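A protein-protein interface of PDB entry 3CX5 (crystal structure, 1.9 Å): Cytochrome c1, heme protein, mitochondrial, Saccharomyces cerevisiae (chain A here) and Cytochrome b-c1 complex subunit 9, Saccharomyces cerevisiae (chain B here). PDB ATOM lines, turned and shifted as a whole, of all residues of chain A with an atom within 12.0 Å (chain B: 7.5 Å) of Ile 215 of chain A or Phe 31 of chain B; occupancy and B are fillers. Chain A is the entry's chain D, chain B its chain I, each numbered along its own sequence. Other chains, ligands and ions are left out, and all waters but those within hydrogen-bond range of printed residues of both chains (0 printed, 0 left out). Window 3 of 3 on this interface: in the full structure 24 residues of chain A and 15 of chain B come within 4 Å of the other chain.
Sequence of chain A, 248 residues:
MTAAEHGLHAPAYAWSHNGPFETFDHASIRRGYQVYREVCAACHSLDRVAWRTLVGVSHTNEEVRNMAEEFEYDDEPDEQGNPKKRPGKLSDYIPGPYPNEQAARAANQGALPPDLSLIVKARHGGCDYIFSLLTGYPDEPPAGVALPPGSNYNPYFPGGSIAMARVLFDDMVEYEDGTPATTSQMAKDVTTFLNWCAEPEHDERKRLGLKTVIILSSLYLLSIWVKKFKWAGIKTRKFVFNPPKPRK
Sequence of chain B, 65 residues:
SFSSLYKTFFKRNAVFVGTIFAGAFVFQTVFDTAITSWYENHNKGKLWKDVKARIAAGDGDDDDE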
ATOM      1  N   PHE A  21     -13.846  10.971 -26.303  1.00  0.00           N
ATOM      2  CA  PHE A  21     -14.083  12.406 -26.448  1.00  0.00           C
ATOM      3  C   PHE A  21     -13.025  13.145 -27.270  1.00  0.00           C
ATOM      4  O   PHE A  21     -13.092  14.366 -27.400  1.00  0.00           O
ATOM      5  CB  PHE A  21     -14.181  13.059 -25.066  1.00  0.00           C
ATOM      6  CG  PHE A  21     -15.067  12.324 -24.099  1.00  0.00           C
ATOM      7  CD1 PHE A  21     -14.564  11.885 -22.876  1.00  0.00           C
ATOM      8  CD2 PHE A  21     -16.401  12.069 -24.405  1.00  0.00           C
ATOM      9  CE1 PHE A  21     -15.377  11.203 -21.971  1.00  0.00           C
ATOM     10  CE2 PHE A  21     -17.222  11.390 -23.512  1.00  0.00           C
ATOM     11  CZ  PHE A  21     -16.714  10.954 -22.291  1.00  0.00           C
ATOM     12  N   GLU A 204     -16.794  14.062 -36.236  1.00  0.00           N
ATOM     13  CA  GLU A 204     -18.242  14.225 -36.169  1.00  0.00           C
ATOM     14  C   GLU A 204     -18.925  12.986 -35.578  1.00  0.00           C
ATOM     15  O   GLU A 204     -19.867  13.112 -34.804  1.00  0.00           O
ATOM     16  CB  GLU A 204     -18.806  14.555 -37.555  1.00  0.00           C
ATOM     17  CG  GLU A 204     -20.322  14.741 -37.599  1.00  0.00           C
ATOM     18  CD  GLU A 204     -20.841  15.921 -36.755  1.00  0.00           C
ATOM     19  OE1 GLU A 204     -22.076  16.026 -36.601  1.00  0.00           O
ATOM     20  OE2 GLU A 204     -20.039  16.738 -36.251  1.00  0.00           O
ATOM     21  N   ARG A 205     -18.410  11.800 -35.908  1.00  0.00           N
ATOM     22  CA  ARG A 205     -18.954  10.542 -35.400  1.00  0.00           C
ATOM     23  C   ARG A 205     -18.876  10.481 -33.876  1.00  0.00           C
ATOM     24  O   ARG A 205     -19.840  10.086 -33.208  1.00  0.00           O
ATOM     25  CB  ARG A 205     -18.207   9.346 -35.999  1.00  0.00           C
ATOM     26  CG  ARG A 205     -18.482   8.029 -35.270  1.00  0.00           C
ATOM     27  CD  ARG A 205     -17.995   6.789 -36.035  1.00  0.00           C
ATOM     28  NE  ARG A 205     -16.598   6.826 -36.464  1.00  0.00           N
ATOM     29  CZ  ARG A 205     -15.544   6.621 -35.677  1.00  0.00           C
ATOM     30  NH1 ARG A 205     -14.328   6.661 -36.198  1.00  0.00           N
ATOM     31  NH2 ARG A 205     -15.695   6.404 -34.373  1.00  0.00           N
ATOM     32  N   LYS A 206     -17.733  10.882 -33.324  1.00  0.00           N
ATOM     33  CA  LYS A 206     -17.571  10.859 -31.879  1.00  0.00           C
ATOM     34  C   LYS A 206     -18.453  11.895 -31.203  1.00  0.00           C
ATOM     35  O   LYS A 206     -18.973  11.653 -30.113  1.00  0.00           O
ATOM     36  CB  LYS A 206     -16.110  11.046 -31.484  1.00  0.00           C
ATOM     37  CG  LYS A 206     -15.258   9.808 -31.688  1.00  0.00           C
ATOM     38  CD  LYS A 206     -13.869  10.061 -31.161  1.00  0.00           C
ATOM     39  CE  LYS A 206     -12.992   8.854 -31.271  1.00  0.00           C
ATOM     40  NZ  LYS A 206     -11.643   9.169 -30.747  1.00  0.00           N
ATOM     41  N   ARG A 207     -18.628  13.044 -31.852  1.00  0.00           N
ATOM     42  CA  ARG A 207     -19.484  14.092 -31.297  1.00  0.00           C
ATOM     43  C   ARG A 207     -20.943  13.610 -31.250  1.00  0.00           C
ATOM     44  O   ARG A 207     -21.630  13.797 -30.244  1.00  0.00           O
ATOM     45  CB  ARG A 207     -19.383  15.357 -32.140  1.00  0.00           C
ATOM     46  CG  ARG A 207     -20.209  16.500 -31.604  1.00  0.00           C
ATOM     47  CD  ARG A 207     -20.370  17.581 -32.644  1.00  0.00           C
ATOM     48  NE  ARG A 207     -21.648  18.245 -32.451  1.00  0.00           N
ATOM     49  CZ  ARG A 207     -22.720  18.047 -33.207  1.00  0.00           C
ATOM     50  NH1 ARG A 207     -23.830  18.691 -32.930  1.00  0.00           N
ATOM     51  NH2 ARG A 207     -22.669  17.259 -34.268  1.00  0.00           N
ATOM     52  N   LEU A 208     -21.406  12.980 -32.334  1.00  0.00           N
ATOM     53  CA  LEU A 208     -22.774  12.460 -32.396  1.00  0.00           C
ATOM     54  C   LEU A 208     -22.928  11.327 -31.395  1.00  0.00           C
ATOM     55  O   LEU A 208     -23.999  11.127 -30.815  1.00  0.00           O
ATOM     56  CB  LEU A 208     -23.110  11.949 -33.802  1.00  0.00           C
ATOM     57  CG  LEU A 208     -23.197  12.981 -34.925  1.00  0.00           C
ATOM     58  CD1 LEU A 208     -23.637  12.303 -36.208  1.00  0.00           C
ATOM     59  CD2 LEU A 208     -24.166  14.088 -34.559  1.00  0.00           C
ATOM     60  N   GLY A 209     -21.844  10.582 -31.202  1.00  0.00           N
ATOM     61  CA  GLY A 209     -21.859   9.479 -30.263  1.00  0.00           C
ATOM     62  C   GLY A 209     -22.118   9.961 -28.847  1.00  0.00           C
ATOM     63  O   GLY A 209     -22.831   9.306 -28.097  1.00  0.00           O
ATOM     64  N   LEU A 210     -21.570  11.121 -28.492  1.00  0.00           N
ATOM     65  CA  LEU A 210     -21.763  11.670 -27.148  1.00  0.00           C
ATOM     66  C   LEU A 210     -23.236  12.021 -26.948  1.00  0.00           C
ATOM     67  O   LEU A 210     -23.822  11.704 -25.915  1.00  0.00           O
ATOM     68  CB  LEU A 210     -20.874  12.905 -26.924  1.00  0.00           C
ATOM     69  CG  LEU A 210     -20.922  13.536 -25.523  1.00  0.00           C
ATOM     70  CD1 LEU A 210     -20.552  12.505 -24.458  1.00  0.00           C
ATOM     71  CD2 LEU A 210     -19.982  14.734 -25.462  1.00  0.00           C
ATOM     72  N   LYS A 211     -23.833  12.647 -27.956  1.00  0.00           N
ATOM     73  CA  LYS A 211     -25.241  13.021 -27.899  1.00  0.00           C
ATOM     74  C   LYS A 211     -26.121  11.775 -27.780  1.00  0.00           C
ATOM     75  O   LYS A 211     -27.028  11.711 -26.940  1.00  0.00           O
ATOM     76  CB  LYS A 211     -25.642  13.790 -29.162  1.00  0.00           C
ATOM     77  CG  LYS A 211     -24.898  15.098 -29.375  1.00  0.00           C
ATOM     78  CD  LYS A 211     -25.472  15.875 -30.553  1.00  0.00           C
ATOM     79  CE  LYS A 211     -26.928  16.244 -30.309  1.00  0.00           C
ATOM     80  NZ  LYS A 211     -27.550  16.908 -31.487  1.00  0.00           N
ATOM     81  N   THR A 212     -25.809  10.780 -28.610  1.00  0.00           N
ATOM     82  CA  THR A 212     -26.549   9.525 -28.665  1.00  0.00           C
ATOM     83  C   THR A 212     -26.478   8.685 -27.391  1.00  0.00           C
ATOM     84  O   THR A 212     -27.498   8.171 -26.936  1.00  0.00           O
ATOM     85  CB  THR A 212     -26.108   8.685 -29.891  1.00  0.00           C
ATOM     86  OG1 THR A 212     -26.180   9.501 -31.067  1.00  0.00           O
ATOM     87  CG2 THR A 212     -27.025   7.496 -30.091  1.00  0.00           C
ATOM     88  N   VAL A 213     -25.293   8.547 -26.805  1.00  0.00           N
ATOM     89  CA  VAL A 213     -25.161   7.761 -25.581  1.00  0.00           C
ATOM     90  C   VAL A 213     -25.818   8.449 -24.381  1.00  0.00           C
ATOM     91  O   VAL A 213     -26.413   7.789 -23.528  1.00  0.00           O
ATOM     92  CB  VAL A 213     -23.681   7.408 -25.291  1.00  0.00           C
ATOM     93  CG1 VAL A 213     -23.533   6.781 -23.913  1.00  0.00           C
ATOM     94  CG2 VAL A 213     -23.180   6.434 -26.355  1.00  0.00           C
ATOM     95  N   ILE A 214     -25.738   9.777 -24.330  1.00  0.00           N
ATOM     96  CA  ILE A 214     -26.360  10.515 -23.235  1.00  0.00           C
ATOM     97  C   ILE A 214     -27.879  10.368 -23.273  1.00  0.00           C
ATOM     98  O   ILE A 214     -28.492  10.002 -22.274  1.00  0.00           O
ATOM     99  CB  ILE A 214     -25.966  12.009 -23.250  1.00  0.00           C
ATOM    100  CG1 ILE A 214     -24.482  12.152 -22.877  1.00  0.00           C
ATOM    101  CG2 ILE A 214     -26.837  12.796 -22.274  1.00  0.00           C
ATOM    102  CD1 ILE A 214     -23.932  13.563 -23.035  1.00  0.00           C
ATOM    103  N   ILE A 215     -28.474  10.604 -24.440  1.00  0.00           N
ATOM    104  CA  ILE A 215     -29.923  10.489 -24.604  1.00  0.00           C
ATOM    105  C   ILE A 215     -30.406   9.062 -24.320  1.00  0.00           C
ATOM    106  O   ILE A 215     -31.390   8.863 -23.603  1.00  0.00           O
ATOM    107  CB  ILE A 215     -30.363  10.928 -26.024  1.00  0.00           C
ATOM    108  CG1 ILE A 215     -30.159  12.438 -26.189  1.00  0.00           C
ATOM    109  CG2 ILE A 215     -31.837  10.583 -26.274  1.00  0.00           C
ATOM    110  CD1 ILE A 215     -30.405  12.935 -27.601  1.00  0.00           C
ATOM    111  N   LEU A 216     -29.696   8.073 -24.863  1.00  0.00           N
ATOM    112  CA  LEU A 216     -30.064   6.676 -24.659  1.00  0.00           C
ATOM    113  C   LEU A 216     -29.887   6.195 -23.221  1.00  0.00           C
ATOM    114  O   LEU A 216     -30.691   5.400 -22.731  1.00  0.00           O
ATOM    115  CB  LEU A 216     -29.316   5.774 -25.641  1.00  0.00           C
ATOM    116  CG  LEU A 216     -29.883   5.883 -27.062  1.00  0.00           C
ATOM    117  CD1 LEU A 216     -29.007   5.152 -28.065  1.00  0.00           C
ATOM    118  CD2 LEU A 216     -31.321   5.340 -27.076  1.00  0.00           C
ATOM    119  N   SER A 217     -28.846   6.675 -22.542  1.00  0.00           N
ATOM    120  CA  SER A 217     -28.621   6.286 -21.155  1.00  0.00           C
ATOM    121  C   SER A 217     -29.762   6.817 -20.310  1.00  0.00           C
ATOM    122  O   SER A 217     -30.257   6.121 -19.422  1.00  0.00           O
ATOM    123  CB  SER A 217     -27.290   6.837 -20.623  1.00  0.00           C
ATOM    124  OG  SER A 217     -26.191   6.145 -21.173  1.00  0.00           O
ATOM    125  N   SER A 218     -30.175   8.055 -20.583  1.00  0.00           N
ATOM    126  CA  SER A 218     -31.274   8.676 -19.837  1.00  0.00           C
ATOM    127  C   SER A 218     -32.571   7.925 -20.098  1.00  0.00           C
ATOM    128  O   SER A 218     -33.324   7.637 -19.167  1.00  0.00           O
ATOM    129  CB  SER A 218     -31.451  10.143 -20.239  1.00  0.00           C
ATOM    130  OG  SER A 218     -30.269  10.884 -19.990  1.00  0.00           O
ATOM    131  N   LEU A 219     -32.810   7.599 -21.368  1.00  0.00           N
ATOM    132  CA  LEU A 219     -34.007   6.867 -21.781  1.00  0.00           C
ATOM    133  C   LEU A 219     -34.064   5.511 -21.081  1.00  0.00           C
ATOM    134  O   LEU A 219     -35.117   5.101 -20.610  1.00  0.00           O
ATOM    135  CB  LEU A 219     -34.018   6.687 -23.308  1.00  0.00           C
ATOM    136  CG  LEU A 219     -35.002   7.443 -24.214  1.00  0.00           C
ATOM    137  CD1 LEU A 219     -35.858   8.439 -23.475  1.00  0.00           C
ATOM    138  CD2 LEU A 219     -34.262   8.092 -25.353  1.00  0.00           C
ATOM    139  N   TYR A 220     -32.922   4.831 -21.007  1.00  0.00           N
ATOM    140  CA  TYR A 220     -32.835   3.532 -20.348  1.00  0.00           C
ATOM    141  C   TYR A 220     -33.209   3.635 -18.860  1.00  0.00           C
ATOM    142  O   TYR A 220     -34.048   2.869 -18.376  1.00  0.00           O
ATOM    143  CB  TYR A 220     -31.423   2.956 -20.505  1.00  0.00           C
ATOM    144  CG  TYR A 220     -31.162   1.692 -19.710  1.00  0.00           C
ATOM    145  CD1 TYR A 220     -31.981   0.563 -19.846  1.00  0.00           C
ATOM    146  CD2 TYR A 220     -30.092   1.622 -18.825  1.00  0.00           C
ATOM    147  CE1 TYR A 220     -31.734  -0.605 -19.114  1.00  0.00           C
ATOM    148  CE2 TYR A 220     -29.834   0.465 -18.089  1.00  0.00           C
ATOM    149  CZ  TYR A 220     -30.655  -0.643 -18.234  1.00  0.00           C
ATOM    150  OH  TYR A 220     -30.384  -1.773 -17.492  1.00  0.00           O
ATOM    151  N   LEU A 221     -32.617   4.602 -18.153  1.00  0.00           N
ATOM    152  CA  LEU A 221     -32.893   4.789 -16.723  1.00  0.00           C
ATOM    153  C   LEU A 221     -34.343   5.204 -16.473  1.00  0.00           C
ATOM    154  O   LEU A 221     -34.985   4.736 -15.526  1.00  0.00           O
ATOM    155  CB  LEU A 221     -31.938   5.826 -16.119  1.00  0.00           C
ATOM    156  CG  LEU A 221     -30.446   5.475 -16.154  1.00  0.00           C
ATOM    157  CD1 LEU A 221     -29.615   6.655 -15.636  1.00  0.00           C
ATOM    158  CD2 LEU A 221     -30.183   4.211 -15.334  1.00  0.00           C
ATOM    159  N   LEU A 222     -34.843   6.088 -17.330  1.00  0.00           N
ATOM    160  CA  LEU A 222     -36.215   6.578 -17.258  1.00  0.00           C
ATOM    161  C   LEU A 222     -37.182   5.411 -17.444  1.00  0.00           C
ATOM    162  O   LEU A 222     -38.135   5.262 -16.688  1.00  0.00           O
ATOM    163  CB  LEU A 222     -36.444   7.615 -18.363  1.00  0.00           C
ATOM    164  CG  LEU A 222     -36.499   9.125 -18.079  1.00  0.00           C
ATOM    165  CD1 LEU A 222     -35.761   9.503 -16.816  1.00  0.00           C
ATOM    166  CD2 LEU A 222     -35.963   9.891 -19.286  1.00  0.00           C
ATOM    167  N   SER A 223     -36.896   4.557 -18.427  1.00  0.00           N
ATOM    168  CA  SER A 223     -37.753   3.409 -18.720  1.00  0.00           C
ATOM    169  C   SER A 223     -37.838   2.417 -17.564  1.00  0.00           C
ATOM    170  O   SER A 223     -38.880   1.802 -17.344  1.00  0.00           O
ATOM    171  CB  SER A 223     -37.306   2.714 -20.012  1.00  0.00           C
ATOM    172  OG  SER A 223     -36.072   2.041 -19.849  1.00  0.00           O
ATOM    173  N   ILE A 224     -36.750   2.278 -16.811  1.00  0.00           N
ATOM    174  CA  ILE A 224     -36.738   1.377 -15.664  1.00  0.00           C
ATOM    175  C   ILE A 224     -37.691   1.917 -14.595  1.00  0.00           C
ATOM    176  O   ILE A 224     -38.534   1.189 -14.080  1.00  0.00           O
ATOM    177  CB  ILE A 224     -35.313   1.233 -15.078  1.00  0.00           C
ATOM    178  CG1 ILE A 224     -34.434   0.452 -16.051  1.00  0.00           C
ATOM    179  CG2 ILE A 224     -35.354   0.523 -13.730  1.00  0.00           C
ATOM    180  CD1 ILE A 224     -32.987   0.396 -15.636  1.00  0.00           C
ATOM    181  N   PHE B  25     -38.506  19.957 -29.346  1.00  0.00           N
ATOM    182  CA  PHE B  25     -37.932  20.900 -30.304  1.00  0.00           C
ATOM    183  C   PHE B  25     -36.927  21.804 -29.592  1.00  0.00           C
ATOM    184  O   PHE B  25     -35.829  22.041 -30.102  1.00  0.00           O
ATOM    185  CB  PHE B  25     -39.023  21.746 -30.972  1.00  0.00           C
ATOM    186  CG  PHE B  25     -40.012  20.946 -31.784  1.00  0.00           C
ATOM    187  CD1 PHE B  25     -41.280  21.458 -32.055  1.00  0.00           C
ATOM    188  CD2 PHE B  25     -39.680  19.683 -32.279  1.00  0.00           C
ATOM    189  CE1 PHE B  25     -42.204  20.724 -32.810  1.00  0.00           C
ATOM    190  CE2 PHE B  25     -40.595  18.943 -33.032  1.00  0.00           C
ATOM    191  CZ  PHE B  25     -41.858  19.461 -33.298  1.00  0.00           C
ATOM    192  N   VAL B  26     -37.301  22.288 -28.409  1.00  0.00           N
ATOM    193  CA  VAL B  26     -36.425  23.148 -27.617  1.00  0.00           C
ATOM    194  C   VAL B  26     -35.225  22.336 -27.135  1.00  0.00           C
ATOM    195  O   VAL B  26     -34.087  22.808 -27.190  1.00  0.00           O
ATOM    196  CB  VAL B  26     -37.161  23.745 -26.388  1.00  0.00           C
ATOM    197  CG1 VAL B  26     -36.198  24.564 -25.539  1.00  0.00           C
ATOM    198  CG2 VAL B  26     -38.317  24.624 -26.844  1.00  0.00           C
ATOM    199  N   PHE B  27     -35.480  21.108 -26.683  1.00  0.00           N
ATOM    200  CA  PHE B  27     -34.408  20.240 -26.208  1.00  0.00           C
ATOM    201  C   PHE B  27     -33.337  20.047 -27.280  1.00  0.00           C
ATOM    202  O   PHE B  27     -32.146  20.181 -27.003  1.00  0.00           O
ATOM    203  CB  PHE B  27     -34.945  18.868 -25.779  1.00  0.00           C
ATOM    204  CG  PHE B  27     -33.860  17.878 -25.450  1.00  0.00           C
ATOM    205  CD1 PHE B  27     -33.267  17.867 -24.187  1.00  0.00           C
ATOM    206  CD2 PHE B  27     -33.376  17.006 -26.427  1.00  0.00           C
ATOM    207  CE1 PHE B  27     -32.207  17.014 -23.902  1.00  0.00           C
ATOM    208  CE2 PHE B  27     -32.315  16.146 -26.154  1.00  0.00           C
ATOM    209  CZ  PHE B  27     -31.726  16.149 -24.888  1.00  0.00           C
ATOM    210  N   GLN B  28     -33.777  19.735 -28.497  1.00  0.00           N
ATOM    211  CA  GLN B  28     -32.880  19.498 -29.622  1.00  0.00           C
ATOM    212  C   GLN B  28     -31.892  20.638 -29.876  1.00  0.00           C
ATOM    213  O   GLN B  28     -30.710  20.396 -30.111  1.00  0.00           O
ATOM    214  CB  GLN B  28     -33.690  19.198 -30.885  1.00  0.00           C
ATOM    215  CG  GLN B  28     -32.927  18.415 -31.949  1.00  0.00           C
ATOM    216  CD  GLN B  28     -33.847  17.592 -32.855  1.00  0.00           C
ATOM    217  OE1 GLN B  28     -34.196  16.444 -32.539  1.00  0.00           O
ATOM    218  NE2 GLN B  28     -34.238  18.174 -33.984  1.00  0.00           N
ATOM    219  N   THR B  29     -32.373  21.875 -29.786  1.00  0.00           N
ATOM    220  CA  THR B  29     -31.535  23.052 -30.001  1.00  0.00           C
ATOM    221  C   THR B  29     -30.529  23.271 -28.866  1.00  0.00           C
ATOM    222  O   THR B  29     -29.320  23.343 -29.098  1.00  0.00           O
ATOM    223  CB  THR B  29     -32.401  24.322 -30.150  1.00  0.00           C
ATOM    224  OG1 THR B  29     -33.281  24.170 -31.269  1.00  0.00           O
ATOM    225  CG2 THR B  29     -31.526  25.556 -30.365  1.00  0.00           C
ATOM    226  N   VAL B  30     -31.038  23.374 -27.643  1.00  0.00           N
ATOM    227  CA  VAL B  30     -30.201  23.607 -26.472  1.00  0.00           C
ATOM    228  C   VAL B  30     -29.189  22.495 -26.231  1.00  0.00           C
ATOM    229  O   VAL B  30     -28.018  22.760 -25.925  1.00  0.00           O
ATOM    230  CB  VAL B  30     -31.065  23.810 -25.211  1.00  0.00           C
ATOM    231  CG1 VAL B  30     -30.188  23.931 -23.970  1.00  0.00           C
ATOM    232  CG2 VAL B  30     -31.918  25.067 -25.371  1.00  0.00           C
ATOM    233  N   PHE B  31     -29.637  21.252 -26.385  1.00  0.00           N
ATOM    234  CA  PHE B  31     -28.772  20.103 -26.177  1.00  0.00           C
ATOM    235  C   PHE B  31     -27.621  20.086 -27.180  1.00  0.00           C
ATOM    236  O   PHE B  31     -26.473  19.858 -26.804  1.00  0.00           O
ATOM    237  CB  PHE B  31     -29.585  18.805 -26.264  1.00  0.00           C
ATOM    238  CG  PHE B  31     -28.808  17.572 -25.902  1.00  0.00           C
ATOM    239  CD1 PHE B  31     -28.369  17.366 -24.598  1.00  0.00           C
ATOM    240  CD2 PHE B  31     -28.526  16.608 -26.861  1.00  0.00           C
ATOM    241  CE1 PHE B  31     -27.662  16.216 -24.257  1.00  0.00           C
ATOM    242  CE2 PHE B  31     -27.819  15.456 -26.529  1.00  0.00           C
ATOM    243  CZ  PHE B  31     -27.387  15.259 -25.227  1.00  0.00           C
ATOM    244  N   ASP B  32     -27.920  20.365 -28.446  1.00  0.00           N
ATOM    245  CA  ASP B  32     -26.892  20.359 -29.481  1.00  0.00           C
ATOM    246  C   ASP B  32     -25.809  21.412 -29.239  1.00  0.00           C
ATOM    247  O   ASP B  32     -24.618  21.131 -29.381  1.00  0.00           O
ATOM    248  CB  ASP B  32     -27.512  20.565 -30.863  1.00  0.00           C
ATOM    249  CG  ASP B  32     -26.519  20.321 -31.982  1.00  0.00           C
ATOM    250  OD1 ASP B  32     -26.163  19.148 -32.209  1.00  0.00           O
ATOM    251  OD2 ASP B  32     -26.086  21.295 -32.630  1.00  0.00           O
ATOM    252  N   THR B  33     -26.236  22.618 -28.873  1.00  0.00           N
ATOM    253  CA  THR B  33     -25.319  23.723 -28.607  1.00  0.00           C
ATOM    254  C   THR B  33     -24.414  23.414 -27.410  1.00  0.00           C
ATOM    255  O   THR B  33     -23.205  23.642 -27.462  1.00  0.00           O
ATOM    256  CB  THR B  33     -26.107  25.031 -28.338  1.00  0.00           C
ATOM    257  OG1 THR B  33     -26.956  25.311 -29.458  1.00  0.00           O
ATOM    258  CG2 THR B  33     -25.157  26.206 -28.123  1.00  0.00           C
ATOM    259  N   ALA B  34     -25.006  22.875 -26.350  1.00  0.00           N
ATOM    260  CA  ALA B  34     -24.272  22.528 -25.138  1.00  0.00           C
ATOM    261  C   ALA B  34     -23.214  21.452 -25.389  1.00  0.00           C
ATOM    262  O   ALA B  34     -22.069  21.587 -24.948  1.00  0.00           O
ATOM    263  CB  ALA B  34     -25.240  22.070 -24.058  1.00  0.00           C
ATOM    264  N   ILE B  35     -23.602  20.395 -26.104  1.00  0.00           N
ATOM    265  CA  ILE B  35     -22.694  19.291 -26.413  1.00  0.00           C
ATOM    266  C   ILE B  35     -21.557  19.745 -27.314  1.00  0.00           C
ATOM    267  O   ILE B  35     -20.396  19.431 -27.056  1.00  0.00           O
ATOM    268  CB  ILE B  35     -23.434  18.109 -27.097  1.00  0.00           C
ATOM    269  CG1 ILE B  35     -24.456  17.498 -26.138  1.00  0.00           C
ATOM    270  CG2 ILE B  35     -22.441  17.051 -27.555  1.00  0.00           C
ATOM    271  CD1 ILE B  35     -23.863  17.033 -24.819  1.00  0.00           C
ATOM    272  N   THR B  36     -21.898  20.480 -28.368  1.00  0.00           N
ATOM    273  CA  THR B  36     -20.912  20.978 -29.315  1.00  0.00           C
ATOM    274  C   THR B  36     -19.893  21.889 -28.628  1.00  0.00           C
ATOM    275  O   THR B  36     -18.690  21.756 -28.858  1.00  0.00           O
ATOM    276  CB  THR B  36     -21.594  21.711 -30.486  1.00  0.00           C
ATOM    277  OG1 THR B  36     -22.323  20.760 -31.275  1.00  0.00           O
ATOM    278  CG2 THR B  36     -20.570  22.415 -31.368  1.00  0.00           C
ATOM    279  N   SER B  37     -20.372  22.786 -27.766  1.00  0.00           N
ATOM    280  CA  SER B  37     -19.484  23.698 -27.040  1.00  0.00           C
ATOM    281  C   SER B  37     -18.542  22.932 -26.119  1.00  0.00           C
ATOM    282  O   SER B  37     -17.344  23.212 -26.090  1.00  0.00           O
ATOM    283  CB  SER B  37     -20.281  24.722 -26.224  1.00  0.00           C
ATOM    284  OG  SER B  37     -20.914  25.660 -27.075  1.00  0.00           O
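NH1 of Arg 207 of chain A lies within salt-bridge range of OD1 of Asp 32 of chain B.
The side-chain amino group of Lys 211 of chain A lies within salt-bridge range of the side-chain carboxylate of Asp 32 of chain B, 2.7 Å away.
The guanidinium group (NE) of Arg 207 of chain A lies within hydrogen-bond range of the side-chain hydroxyl (OG1) of Thr 36 of chain B (2.9 Å).
Of the printed residues of chain B, Ile 215 of chain A touches Phe 31 (3.8 Å).
Of chain A, only Lys 211, Ile 214 and Ile 215 come within 4 Å of Phe 31 of chain B.
No residue of chain A comes within 4 Å of Val 30 of chain B.
Thr 33 of chain B touches none of the printed residues of chain A.
Of chain A, only Leu 210, Lys 211 and Ile 214 come within 4 Å of Ile 35 of chain B.
Of the printed residues of chain B, Leu 210 of chain A touches Ile 35 (3.97 Å).
Of the printed residues of chain A, Thr 36 of chain B touches Arg 207.
Gly 209 of chain A touches none of the printed residues of chain B.
Lys 206 of chain A touches none of the printed residues of chain B.
The backbone carbonyl oxygen (O) of Asp 32 of chain B sits at hydrogen-bond distance from the side-chain hydroxyl (OG1) of Thr 36 of chain B (3.0 Å).
OE1 of Glu 204 of chain A lies within salt-bridge range of NH2 of Arg 207 of chain A, at 2.7 Å.
The backbone carbonyl oxygen of Ile 214 of chain A lies within hydrogen-bond range of the side-chain hydroxyl of Ser 218 of chain A, 3.0 Å away.
Of the 13 printed residues of chain B, 4 touch a printed residue of chain A.
Hydrophobic or aromatic side chains of chain B that line the printed part of chain A: Phe 31 and Ile 35.
Along chain B the printed residues that touch a printed residue of chain A span positions 31 to 36.
Of the 22 printed residues of chain A, 5 touch a printed residue of chain B.
Hydrophobic or aromatic side chains of chain A within 4 Å of the printed part of chain B: Leu 210, Ile 214 and Ile 215.
Among the printed residues, Asp or Glu carboxylates within 4 Å of a Lys or Arg side-chain nitrogen of the other chain: Arg 207 of chain A with Asp 32 of chain B (2.5 Å) and Lys 211 of chain A with Asp 32 of chain B (2.7 Å).
Among the printed residues, merely in contact across the chains: Leu 210 of chain A with Ile 35 of chain B, Lys 211 of chain A with Phe 31 of chain B, Lys 211 of chain A with Ile 35 of chain B, Ile 214 of chain A with Phe 31 of chain B, Ile 214 of chain A with Ile 35 of chain B and Ile 215 of chain A with Phe 31 of chain B.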
